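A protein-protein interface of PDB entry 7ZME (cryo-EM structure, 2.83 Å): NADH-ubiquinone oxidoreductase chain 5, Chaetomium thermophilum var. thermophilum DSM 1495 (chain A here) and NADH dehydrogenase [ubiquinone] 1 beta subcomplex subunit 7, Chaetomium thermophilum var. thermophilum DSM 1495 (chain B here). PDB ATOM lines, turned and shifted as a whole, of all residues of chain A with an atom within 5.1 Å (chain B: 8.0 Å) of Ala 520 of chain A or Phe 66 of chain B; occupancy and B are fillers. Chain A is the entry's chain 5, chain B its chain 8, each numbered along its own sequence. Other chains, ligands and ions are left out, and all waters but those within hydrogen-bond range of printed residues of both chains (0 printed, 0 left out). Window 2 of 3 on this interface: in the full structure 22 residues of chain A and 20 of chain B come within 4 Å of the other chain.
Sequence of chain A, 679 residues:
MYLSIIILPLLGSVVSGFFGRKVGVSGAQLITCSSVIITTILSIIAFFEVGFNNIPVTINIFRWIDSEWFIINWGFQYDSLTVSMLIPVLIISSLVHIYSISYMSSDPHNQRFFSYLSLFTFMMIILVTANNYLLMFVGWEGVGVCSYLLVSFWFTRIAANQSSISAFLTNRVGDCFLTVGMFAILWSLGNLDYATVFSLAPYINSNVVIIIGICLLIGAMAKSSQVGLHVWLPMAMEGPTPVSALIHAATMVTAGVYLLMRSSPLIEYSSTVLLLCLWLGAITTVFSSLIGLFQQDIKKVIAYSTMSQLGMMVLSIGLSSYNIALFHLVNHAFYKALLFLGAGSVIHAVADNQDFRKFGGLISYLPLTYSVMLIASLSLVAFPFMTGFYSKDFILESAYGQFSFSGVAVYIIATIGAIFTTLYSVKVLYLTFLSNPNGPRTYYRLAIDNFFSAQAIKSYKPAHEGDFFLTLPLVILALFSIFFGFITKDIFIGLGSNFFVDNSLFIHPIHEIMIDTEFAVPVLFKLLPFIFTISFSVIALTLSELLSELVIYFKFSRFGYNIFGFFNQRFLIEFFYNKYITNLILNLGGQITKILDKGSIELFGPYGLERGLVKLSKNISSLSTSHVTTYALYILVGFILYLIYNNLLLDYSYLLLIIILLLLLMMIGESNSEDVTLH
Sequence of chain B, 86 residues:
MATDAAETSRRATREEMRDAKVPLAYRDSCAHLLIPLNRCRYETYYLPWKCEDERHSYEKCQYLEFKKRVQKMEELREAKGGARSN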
ATOM      1  N   PHE A 403      21.231 -26.703 -30.837  1.00  0.00           N
ATOM      2  CA  PHE A 403      22.100 -25.709 -30.211  1.00  0.00           C
ATOM      3  C   PHE A 403      23.495 -26.305 -30.024  1.00  0.00           C
ATOM      4  O   PHE A 403      23.984 -26.528 -28.915  1.00  0.00           O
ATOM      5  CB  PHE A 403      21.493 -25.229 -28.902  1.00  0.00           C
ATOM      6  CG  PHE A 403      20.632 -24.013 -29.058  1.00  0.00           C
ATOM      7  CD1 PHE A 403      19.290 -24.138 -29.349  1.00  0.00           C
ATOM      8  CD2 PHE A 403      21.170 -22.745 -28.933  1.00  0.00           C
ATOM      9  CE1 PHE A 403      18.495 -23.026 -29.502  1.00  0.00           C
ATOM     10  CE2 PHE A 403      20.380 -21.628 -29.084  1.00  0.00           C
ATOM     11  CZ  PHE A 403      19.040 -21.770 -29.371  1.00  0.00           C
ATOM     12  N   ILE A 515      11.241 -29.404 -30.460  1.00  0.00           N
ATOM     13  CA  ILE A 515      10.616 -28.536 -29.466  1.00  0.00           C
ATOM     14  C   ILE A 515      11.418 -27.251 -29.285  1.00  0.00           C
ATOM     15  O   ILE A 515      10.845 -26.167 -29.119  1.00  0.00           O
ATOM     16  CB  ILE A 515      10.421 -29.296 -28.138  1.00  0.00           C
ATOM     17  CG1 ILE A 515       9.545 -28.487 -27.181  1.00  0.00           C
ATOM     18  CG2 ILE A 515      11.755 -29.666 -27.502  1.00  0.00           C
ATOM     19  CD1 ILE A 515       9.045 -29.282 -26.005  1.00  0.00           C
ATOM     20  N   ASP A 516      12.748 -27.341 -29.315  1.00  0.00           N
ATOM     21  CA  ASP A 516      13.565 -26.143 -29.157  1.00  0.00           C
ATOM     22  C   ASP A 516      13.514 -25.261 -30.393  1.00  0.00           C
ATOM     23  O   ASP A 516      13.612 -24.033 -30.281  1.00  0.00           O
ATOM     24  CB  ASP A 516      15.008 -26.529 -28.836  1.00  0.00           C
ATOM     25  CG  ASP A 516      15.191 -26.940 -27.391  1.00  0.00           C
ATOM     26  OD1 ASP A 516      14.192 -27.326 -26.749  1.00  0.00           O
ATOM     27  OD2 ASP A 516      16.335 -26.873 -26.892  1.00  0.00           O
ATOM     28  N   THR A 517      13.369 -25.860 -31.576  1.00  0.00           N
ATOM     29  CA  THR A 517      13.305 -25.074 -32.802  1.00  0.00           C
ATOM     30  C   THR A 517      12.109 -24.133 -32.787  1.00  0.00           C
ATOM     31  O   THR A 517      12.215 -22.972 -33.199  1.00  0.00           O
ATOM     32  CB  THR A 517      13.245 -26.001 -34.016  1.00  0.00           C
ATOM     33  OG1 THR A 517      14.408 -26.837 -34.039  1.00  0.00           O
ATOM     34  CG2 THR A 517      13.182 -25.199 -35.303  1.00  0.00           C
ATOM     35  N   GLU A 518      10.965 -24.611 -32.306  1.00  0.00           N
ATOM     36  CA  GLU A 518       9.771 -23.782 -32.228  1.00  0.00           C
ATOM     37  C   GLU A 518       9.774 -22.845 -31.030  1.00  0.00           C
ATOM     38  O   GLU A 518       8.922 -21.951 -30.966  1.00  0.00           O
ATOM     39  CB  GLU A 518       8.525 -24.669 -32.181  1.00  0.00           C
ATOM     40  CG  GLU A 518       7.275 -24.025 -32.758  1.00  0.00           C
ATOM     41  CD  GLU A 518       6.278 -25.046 -33.272  1.00  0.00           C
ATOM     42  OE1 GLU A 518       6.697 -26.176 -33.597  1.00  0.00           O
ATOM     43  OE2 GLU A 518       5.076 -24.719 -33.350  1.00  0.00           O
ATOM     44  N   PHE A 519      10.698 -23.010 -30.094  1.00  0.00           N
ATOM     45  CA  PHE A 519      10.628 -22.233 -28.861  1.00  0.00           C
ATOM     46  C   PHE A 519      11.910 -21.491 -28.522  1.00  0.00           C
ATOM     47  O   PHE A 519      11.844 -20.358 -28.041  1.00  0.00           O
ATOM     48  CB  PHE A 519      10.259 -23.160 -27.705  1.00  0.00           C
ATOM     49  CG  PHE A 519       8.854 -23.673 -27.764  1.00  0.00           C
ATOM     50  CD1 PHE A 519       7.823 -22.866 -28.206  1.00  0.00           C
ATOM     51  CD2 PHE A 519       8.565 -24.967 -27.375  1.00  0.00           C
ATOM     52  CE1 PHE A 519       6.535 -23.339 -28.257  1.00  0.00           C
ATOM     53  CE2 PHE A 519       7.280 -25.443 -27.426  1.00  0.00           C
ATOM     54  CZ  PHE A 519       6.262 -24.630 -27.866  1.00  0.00           C
ATOM     55  N   ALA A 520      13.074 -22.093 -28.759  1.00  0.00           N
ATOM     56  CA  ALA A 520      14.325 -21.509 -28.292  1.00  0.00           C
ATOM     57  C   ALA A 520      14.930 -20.514 -29.270  1.00  0.00           C
ATOM     58  O   ALA A 520      15.664 -19.615 -28.847  1.00  0.00           O
ATOM     59  CB  ALA A 520      15.345 -22.613 -27.999  1.00  0.00           C
ATOM     60  N   VAL A 521      14.648 -20.654 -30.557  1.00  0.00           N
ATOM     61  CA  VAL A 521      15.255 -19.773 -31.559  1.00  0.00           C
ATOM     62  C   VAL A 521      14.719 -18.357 -31.373  1.00  0.00           C
ATOM     63  O   VAL A 521      13.495 -18.173 -31.243  1.00  0.00           O
ATOM     64  CB  VAL A 521      14.965 -20.291 -32.967  1.00  0.00           C
ATOM     65  CG1 VAL A 521      15.411 -19.279 -34.011  1.00  0.00           C
ATOM     66  CG2 VAL A 521      15.647 -21.633 -33.188  1.00  0.00           C
ATOM     67  N   PRO A 522      15.576 -17.337 -31.343  1.00  0.00           N
ATOM     68  CA  PRO A 522      15.076 -15.960 -31.276  1.00  0.00           C
ATOM     69  C   PRO A 522      14.305 -15.597 -32.536  1.00  0.00           C
ATOM     70  O   PRO A 522      14.526 -16.160 -33.610  1.00  0.00           O
ATOM     71  CB  PRO A 522      16.352 -15.121 -31.134  1.00  0.00           C
ATOM     72  CG  PRO A 522      17.441 -15.989 -31.662  1.00  0.00           C
ATOM     73  CD  PRO A 522      17.046 -17.393 -31.319  1.00  0.00           C
ATOM     74  N   ASP B  28       6.686 -38.292 -23.152  1.00  0.00           N
ATOM     75  CA  ASP B  28       6.962 -37.511 -21.953  1.00  0.00           C
ATOM     76  C   ASP B  28       5.677 -37.109 -21.238  1.00  0.00           C
ATOM     77  O   ASP B  28       4.598 -37.624 -21.548  1.00  0.00           O
ATOM     78  CB  ASP B  28       7.800 -36.282 -22.306  1.00  0.00           C
ATOM     79  CG  ASP B  28       7.014 -35.234 -23.055  1.00  0.00           C
ATOM     80  OD1 ASP B  28       6.209 -35.604 -23.935  1.00  0.00           O
ATOM     81  OD2 ASP B  28       7.215 -34.035 -22.769  1.00  0.00           O
ATOM     82  N   GLU B  59       0.203 -27.456 -27.869  1.00  0.00           N
ATOM     83  CA  GLU B  59       1.333 -26.559 -28.080  1.00  0.00           C
ATOM     84  C   GLU B  59       1.560 -25.655 -26.878  1.00  0.00           C
ATOM     85  O   GLU B  59       2.696 -25.242 -26.622  1.00  0.00           O
ATOM     86  CB  GLU B  59       1.112 -25.721 -29.339  1.00  0.00           C
ATOM     87  CG  GLU B  59       1.561 -26.397 -30.622  1.00  0.00           C
ATOM     88  CD  GLU B  59       2.055 -25.406 -31.658  1.00  0.00           C
ATOM     89  OE1 GLU B  59       2.662 -24.388 -31.265  1.00  0.00           O
ATOM     90  OE2 GLU B  59       1.840 -25.646 -32.865  1.00  0.00           O
ATOM     91  N   LYS B  60       0.499 -25.336 -26.134  1.00  0.00           N
ATOM     92  CA  LYS B  60       0.661 -24.522 -24.935  1.00  0.00           C
ATOM     93  C   LYS B  60       1.429 -25.275 -23.857  1.00  0.00           C
ATOM     94  O   LYS B  60       2.331 -24.714 -23.225  1.00  0.00           O
ATOM     95  CB  LYS B  60      -0.706 -24.085 -24.412  1.00  0.00           C
ATOM     96  CG  LYS B  60      -0.646 -23.158 -23.209  1.00  0.00           C
ATOM     97  CD  LYS B  60      -2.039 -22.725 -22.780  1.00  0.00           C
ATOM     98  CE  LYS B  60      -1.981 -21.726 -21.637  1.00  0.00           C
ATOM     99  NZ  LYS B  60      -1.469 -22.345 -20.384  1.00  0.00           N
ATOM    100  N   CYS B  61       1.092 -26.547 -23.637  1.00  0.00           N
ATOM    101  CA  CYS B  61       1.791 -27.323 -22.620  1.00  0.00           C
ATOM    102  C   CYS B  61       3.226 -27.605 -23.041  1.00  0.00           C
ATOM    103  O   CYS B  61       4.098 -27.825 -22.193  1.00  0.00           O
ATOM    104  CB  CYS B  61       1.038 -28.621 -22.337  1.00  0.00           C
ATOM    105  SG  CYS B  61       1.771 -29.636 -21.035  1.00  0.00           S
ATOM    106  N   GLN B  62       3.488 -27.607 -24.352  1.00  0.00           N
ATOM    107  CA  GLN B  62       4.864 -27.647 -24.831  1.00  0.00           C
ATOM    108  C   GLN B  62       5.652 -26.449 -24.327  1.00  0.00           C
ATOM    109  O   GLN B  62       6.826 -26.579 -23.966  1.00  0.00           O
ATOM    110  CB  GLN B  62       4.894 -27.663 -26.360  1.00  0.00           C
ATOM    111  CG  GLN B  62       4.285 -28.880 -27.029  1.00  0.00           C
ATOM    112  CD  GLN B  62       5.015 -30.161 -26.708  1.00  0.00           C
ATOM    113  OE1 GLN B  62       4.507 -31.003 -25.977  1.00  0.00           O
ATOM    114  NE2 GLN B  62       6.212 -30.319 -27.257  1.00  0.00           N
ATOM    115  N   TYR B  63       5.021 -25.274 -24.309  1.00  0.00           N
ATOM    116  CA  TYR B  63       5.715 -24.044 -23.952  1.00  0.00           C
ATOM    117  C   TYR B  63       6.065 -24.032 -22.468  1.00  0.00           C
ATOM    118  O   TYR B  63       7.189 -23.684 -22.087  1.00  0.00           O
ATOM    119  CB  TYR B  63       4.835 -22.846 -24.323  1.00  0.00           C
ATOM    120  CG  TYR B  63       5.398 -21.469 -24.026  1.00  0.00           C
ATOM    121  CD1 TYR B  63       6.762 -21.261 -23.875  1.00  0.00           C
ATOM    122  CD2 TYR B  63       4.553 -20.374 -23.901  1.00  0.00           C
ATOM    123  CE1 TYR B  63       7.268 -20.002 -23.613  1.00  0.00           C
ATOM    124  CE2 TYR B  63       5.050 -19.113 -23.634  1.00  0.00           C
ATOM    125  CZ  TYR B  63       6.408 -18.934 -23.489  1.00  0.00           C
ATOM    126  OH  TYR B  63       6.909 -17.680 -23.225  1.00  0.00           O
ATOM    127  N   LEU B  64       5.113 -24.420 -21.614  1.00  0.00           N
ATOM    128  CA  LEU B  64       5.340 -24.369 -20.172  1.00  0.00           C
ATOM    129  C   LEU B  64       6.465 -25.303 -19.749  1.00  0.00           C
ATOM    130  O   LEU B  64       7.337 -24.916 -18.962  1.00  0.00           O
ATOM    131  CB  LEU B  64       4.053 -24.711 -19.418  1.00  0.00           C
ATOM    132  CG  LEU B  64       3.015 -23.607 -19.186  1.00  0.00           C
ATOM    133  CD1 LEU B  64       3.598 -22.515 -18.300  1.00  0.00           C
ATOM    134  CD2 LEU B  64       2.480 -23.024 -20.485  1.00  0.00           C
ATOM    135  N   GLU B  65       6.461 -26.540 -20.252  1.00  0.00           N
ATOM    136  CA  GLU B  65       7.548 -27.458 -19.929  1.00  0.00           C
ATOM    137  C   GLU B  65       8.868 -26.970 -20.501  1.00  0.00           C
ATOM    138  O   GLU B  65       9.924 -27.182 -19.896  1.00  0.00           O
ATOM    139  CB  GLU B  65       7.228 -28.861 -20.443  1.00  0.00           C
ATOM    140  CG  GLU B  65       8.191 -29.935 -19.957  1.00  0.00           C
ATOM    141  CD  GLU B  65       8.164 -30.111 -18.450  1.00  0.00           C
ATOM    142  OE1 GLU B  65       7.099 -29.877 -17.840  1.00  0.00           O
ATOM    143  OE2 GLU B  65       9.208 -30.485 -17.876  1.00  0.00           O
ATOM    144  N   PHE B  66       8.827 -26.318 -21.664  1.00  0.00           N
ATOM    145  CA  PHE B  66      10.028 -25.699 -22.210  1.00  0.00           C
ATOM    146  C   PHE B  66      10.533 -24.592 -21.297  1.00  0.00           C
ATOM    147  O   PHE B  66      11.742 -24.475 -21.063  1.00  0.00           O
ATOM    148  CB  PHE B  66       9.739 -25.152 -23.609  1.00  0.00           C
ATOM    149  CG  PHE B  66      10.896 -24.423 -24.225  1.00  0.00           C
ATOM    150  CD1 PHE B  66      11.953 -25.123 -24.775  1.00  0.00           C
ATOM    151  CD2 PHE B  66      10.930 -23.041 -24.246  1.00  0.00           C
ATOM    152  CE1 PHE B  66      13.018 -24.456 -25.341  1.00  0.00           C
ATOM    153  CE2 PHE B  66      11.993 -22.371 -24.804  1.00  0.00           C
ATOM    154  CZ  PHE B  66      13.037 -23.079 -25.353  1.00  0.00           C
ATOM    155  N   LYS B  67       9.622 -23.768 -20.775  1.00  0.00           N
ATOM    156  CA  LYS B  67      10.021 -22.679 -19.887  1.00  0.00           C
ATOM    157  C   LYS B  67      10.627 -23.209 -18.595  1.00  0.00           C
ATOM    158  O   LYS B  67      11.590 -22.636 -18.074  1.00  0.00           O
ATOM    159  CB  LYS B  67       8.828 -21.776 -19.587  1.00  0.00           C
ATOM    160  CG  LYS B  67       8.684 -20.609 -20.546  1.00  0.00           C
ATOM    161  CD  LYS B  67       9.794 -19.592 -20.346  1.00  0.00           C
ATOM    162  CE  LYS B  67       9.682 -18.449 -21.341  1.00  0.00           C
ATOM    163  NZ  LYS B  67       8.487 -17.602 -21.082  1.00  0.00           N
ATOM    164  N   LYS B  68      10.070 -24.290 -18.052  1.00  0.00           N
ATOM    165  CA  LYS B  68      10.671 -24.899 -16.874  1.00  0.00           C
ATOM    166  C   LYS B  68      12.036 -25.501 -17.175  1.00  0.00           C
ATOM    167  O   LYS B  68      12.833 -25.691 -16.252  1.00  0.00           O
ATOM    168  CB  LYS B  68       9.737 -25.963 -16.296  1.00  0.00           C
ATOM    169  CG  LYS B  68       8.461 -25.390 -15.704  1.00  0.00           C
ATOM    170  CD  LYS B  68       7.577 -26.475 -15.117  1.00  0.00           C
ATOM    171  CE  LYS B  68       6.297 -25.884 -14.551  1.00  0.00           C
ATOM    172  NZ  LYS B  68       5.405 -26.928 -13.978  1.00  0.00           N
ATOM    173  N   ARG B  69      12.323 -25.802 -18.441  1.00  0.00           N
ATOM    174  CA  ARG B  69      13.626 -26.331 -18.816  1.00  0.00           C
ATOM    175  C   ARG B  69      14.614 -25.254 -19.247  1.00  0.00           C
ATOM    176  O   ARG B  69      15.785 -25.570 -19.473  1.00  0.00           O
ATOM    177  CB  ARG B  69      13.480 -27.365 -19.937  1.00  0.00           C
ATOM    178  CG  ARG B  69      12.781 -28.648 -19.507  1.00  0.00           C
ATOM    179  CD  ARG B  69      12.734 -29.663 -20.636  1.00  0.00           C
ATOM    180  NE  ARG B  69      11.848 -29.241 -21.714  1.00  0.00           N
ATOM    181  CZ  ARG B  69      12.264 -28.915 -22.933  1.00  0.00           C
ATOM    182  NH1 ARG B  69      11.388 -28.541 -23.852  1.00  0.00           N
ATOM    183  NH2 ARG B  69      13.554 -28.956 -23.232  1.00  0.00           N
ATOM    184  N   VAL B  70      14.180 -24.001 -19.372  1.00  0.00           N
ATOM    185  CA  VAL B  70      15.123 -22.925 -19.655  1.00  0.00           C
ATOM    186  C   VAL B  70      15.467 -22.149 -18.387  1.00  0.00           C
ATOM    187  O   VAL B  70      16.556 -21.575 -18.288  1.00  0.00           O
ATOM    188  CB  VAL B  70      14.582 -21.981 -20.744  1.00  0.00           C
ATOM    189  CG1 VAL B  70      14.371 -22.730 -22.047  1.00  0.00           C
ATOM    190  CG2 VAL B  70      13.308 -21.296 -20.293  1.00  0.00           C
ATOM    191  N   GLN B  71      14.556 -22.121 -17.413  1.00  0.00           N
ATOM    192  CA  GLN B  71      14.822 -21.484 -16.131  1.00  0.00           C
ATOM    193  C   GLN B  71      15.755 -22.312 -15.259  1.00  0.00           C
ATOM    194  O   GLN B  71      16.368 -21.763 -14.337  1.00  0.00           O
ATOM    195  CB  GLN B  71      13.490 -21.222 -15.415  1.00  0.00           C
ATOM    196  CG  GLN B  71      13.562 -20.387 -14.141  1.00  0.00           C
ATOM    197  CD  GLN B  71      13.866 -21.216 -12.908  1.00  0.00           C
ATOM    198  OE1 GLN B  71      13.516 -22.393 -12.835  1.00  0.00           O
ATOM    199  NE2 GLN B  71      14.521 -20.603 -11.929  1.00  0.00           N
ATOM    200  N   LYS B  72      15.905 -23.605 -15.549  1.00  0.00           N
ATOM    201  CA  LYS B  72      16.710 -24.476 -14.703  1.00  0.00           C
ATOM    202  C   LYS B  72      18.205 -24.230 -14.851  1.00  0.00           C
ATOM    203  O   LYS B  72      18.982 -24.717 -14.021  1.00  0.00           O
ATOM    204  CB  LYS B  72      16.385 -25.941 -15.005  1.00  0.00           C
ATOM    205  CG  LYS B  72      16.678 -26.891 -13.853  1.00  0.00           C
ATOM    206  CD  LYS B  72      15.866 -28.171 -13.966  1.00  0.00           C
ATOM    207  CE  LYS B  72      16.466 -29.123 -14.985  1.00  0.00           C
ATOM    208  NZ  LYS B  72      17.745 -29.716 -14.508  1.00  0.00           N
ATOM    209  N   MET B  73      18.633 -23.496 -15.877  1.00  0.00           N
ATOM    210  CA  MET B  73      20.033 -23.108 -15.980  1.00  0.00           C
ATOM    211  C   MET B  73      20.322 -21.743 -15.375  1.00  0.00           C
ATOM    212  O   MET B  73      21.495 -21.373 -15.264  1.00  0.00           O
ATOM    213  CB  MET B  73      20.499 -23.108 -17.436  1.00  0.00           C
ATOM    214  CG  MET B  73      20.760 -24.482 -17.994  1.00  0.00           C
ATOM    215  SD  MET B  73      19.194 -25.300 -18.274  1.00  0.00           S
ATOM    216  CE  MET B  73      18.693 -24.383 -19.716  1.00  0.00           C
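NZ of Lys 67 of chain B lies within hydrogen-bond range of OH of Tyr 63 of chain B, 2.7 Å away. The guanidinium group (NE) of Arg 69 of chain B lies close to the backbone carbonyl oxygen (O) of Glu 65 of chain B (3.4 Å).
Of the 9 printed residues of chain A, 5 touch a printed residue of chain B. Hydrophobic or aromatic side chains of chain A that line the printed part of chain B: Ile 515, Phe 519 and Ala 520. Along chain A the printed residues that touch a printed residue of chain B span positions 515 to 520. Hydrophobic or aromatic side chains of chain B that line the printed part of chain A: Phe 66. Among the printed residues, Asp or Glu carboxylates within 4 Å of a Lys or Arg side-chain nitrogen of the other chain: Asp 516 of chain A with Arg 69 of chain B.
Ala 520 of chain A touches one residue of chain B. Phe 66 of chain B touches just these residues of chain A: Asp 516, Phe 519 and Ala 520. Of the printed residues of chain A, Glu 59 of chain B touches Glu 518 (3.2 Å) and Phe 519 (3.8 Å). Printed residues of chain A within 4 Å of Arg 69 of chain B: Ile 515 and Asp 516. Of the printed residues of chain B, Ile 515 of chain A touches Gln 62 (3.3 Å) and Arg 69 (3.3 Å). Thr 517 of chain A touches none of the printed residues of chain B. The nearest residue of chain B that does not touch Ala 520 of chain A is Val 70 of chain B (6.0 Å). The nearest residue of chain A that does not touch Phe 66 of chain B is Ile 515 of chain A (4.6 Å).
OE2 of Glu 518 of chain A sits close to OE1 of Glu 59 of chain B, at 3.2 Å. OD1 of Asp 516 of chain A is in salt-bridge range of NH2 of Arg 69 of chain B, 3.9 Å away.
Gln 62 of chain B touches Ile 515 of chain A. Arg 69 of chain B touches Ile 515 of chain A (NH1 to CD1, 3.3 Å). Asp 516 of chain A touches Phe 66 of chain B (OD1 to CE1, 3.4 Å). CZ of Phe 519 of chain A touches O of Glu 59 of chain B (3.8 Å). Phe 519 of chain A touches Gln 62 of chain B (CE2 to CB, 3.4 Å). Phe 519 of chain A touches Tyr 63 of chain B (CZ to N, 3.8 Å). Phe 66 of chain B touches Phe 519 of chain A (CE2 to CB, 3.5 Å). Ala 520 of chain A touches Phe 66 of chain B.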
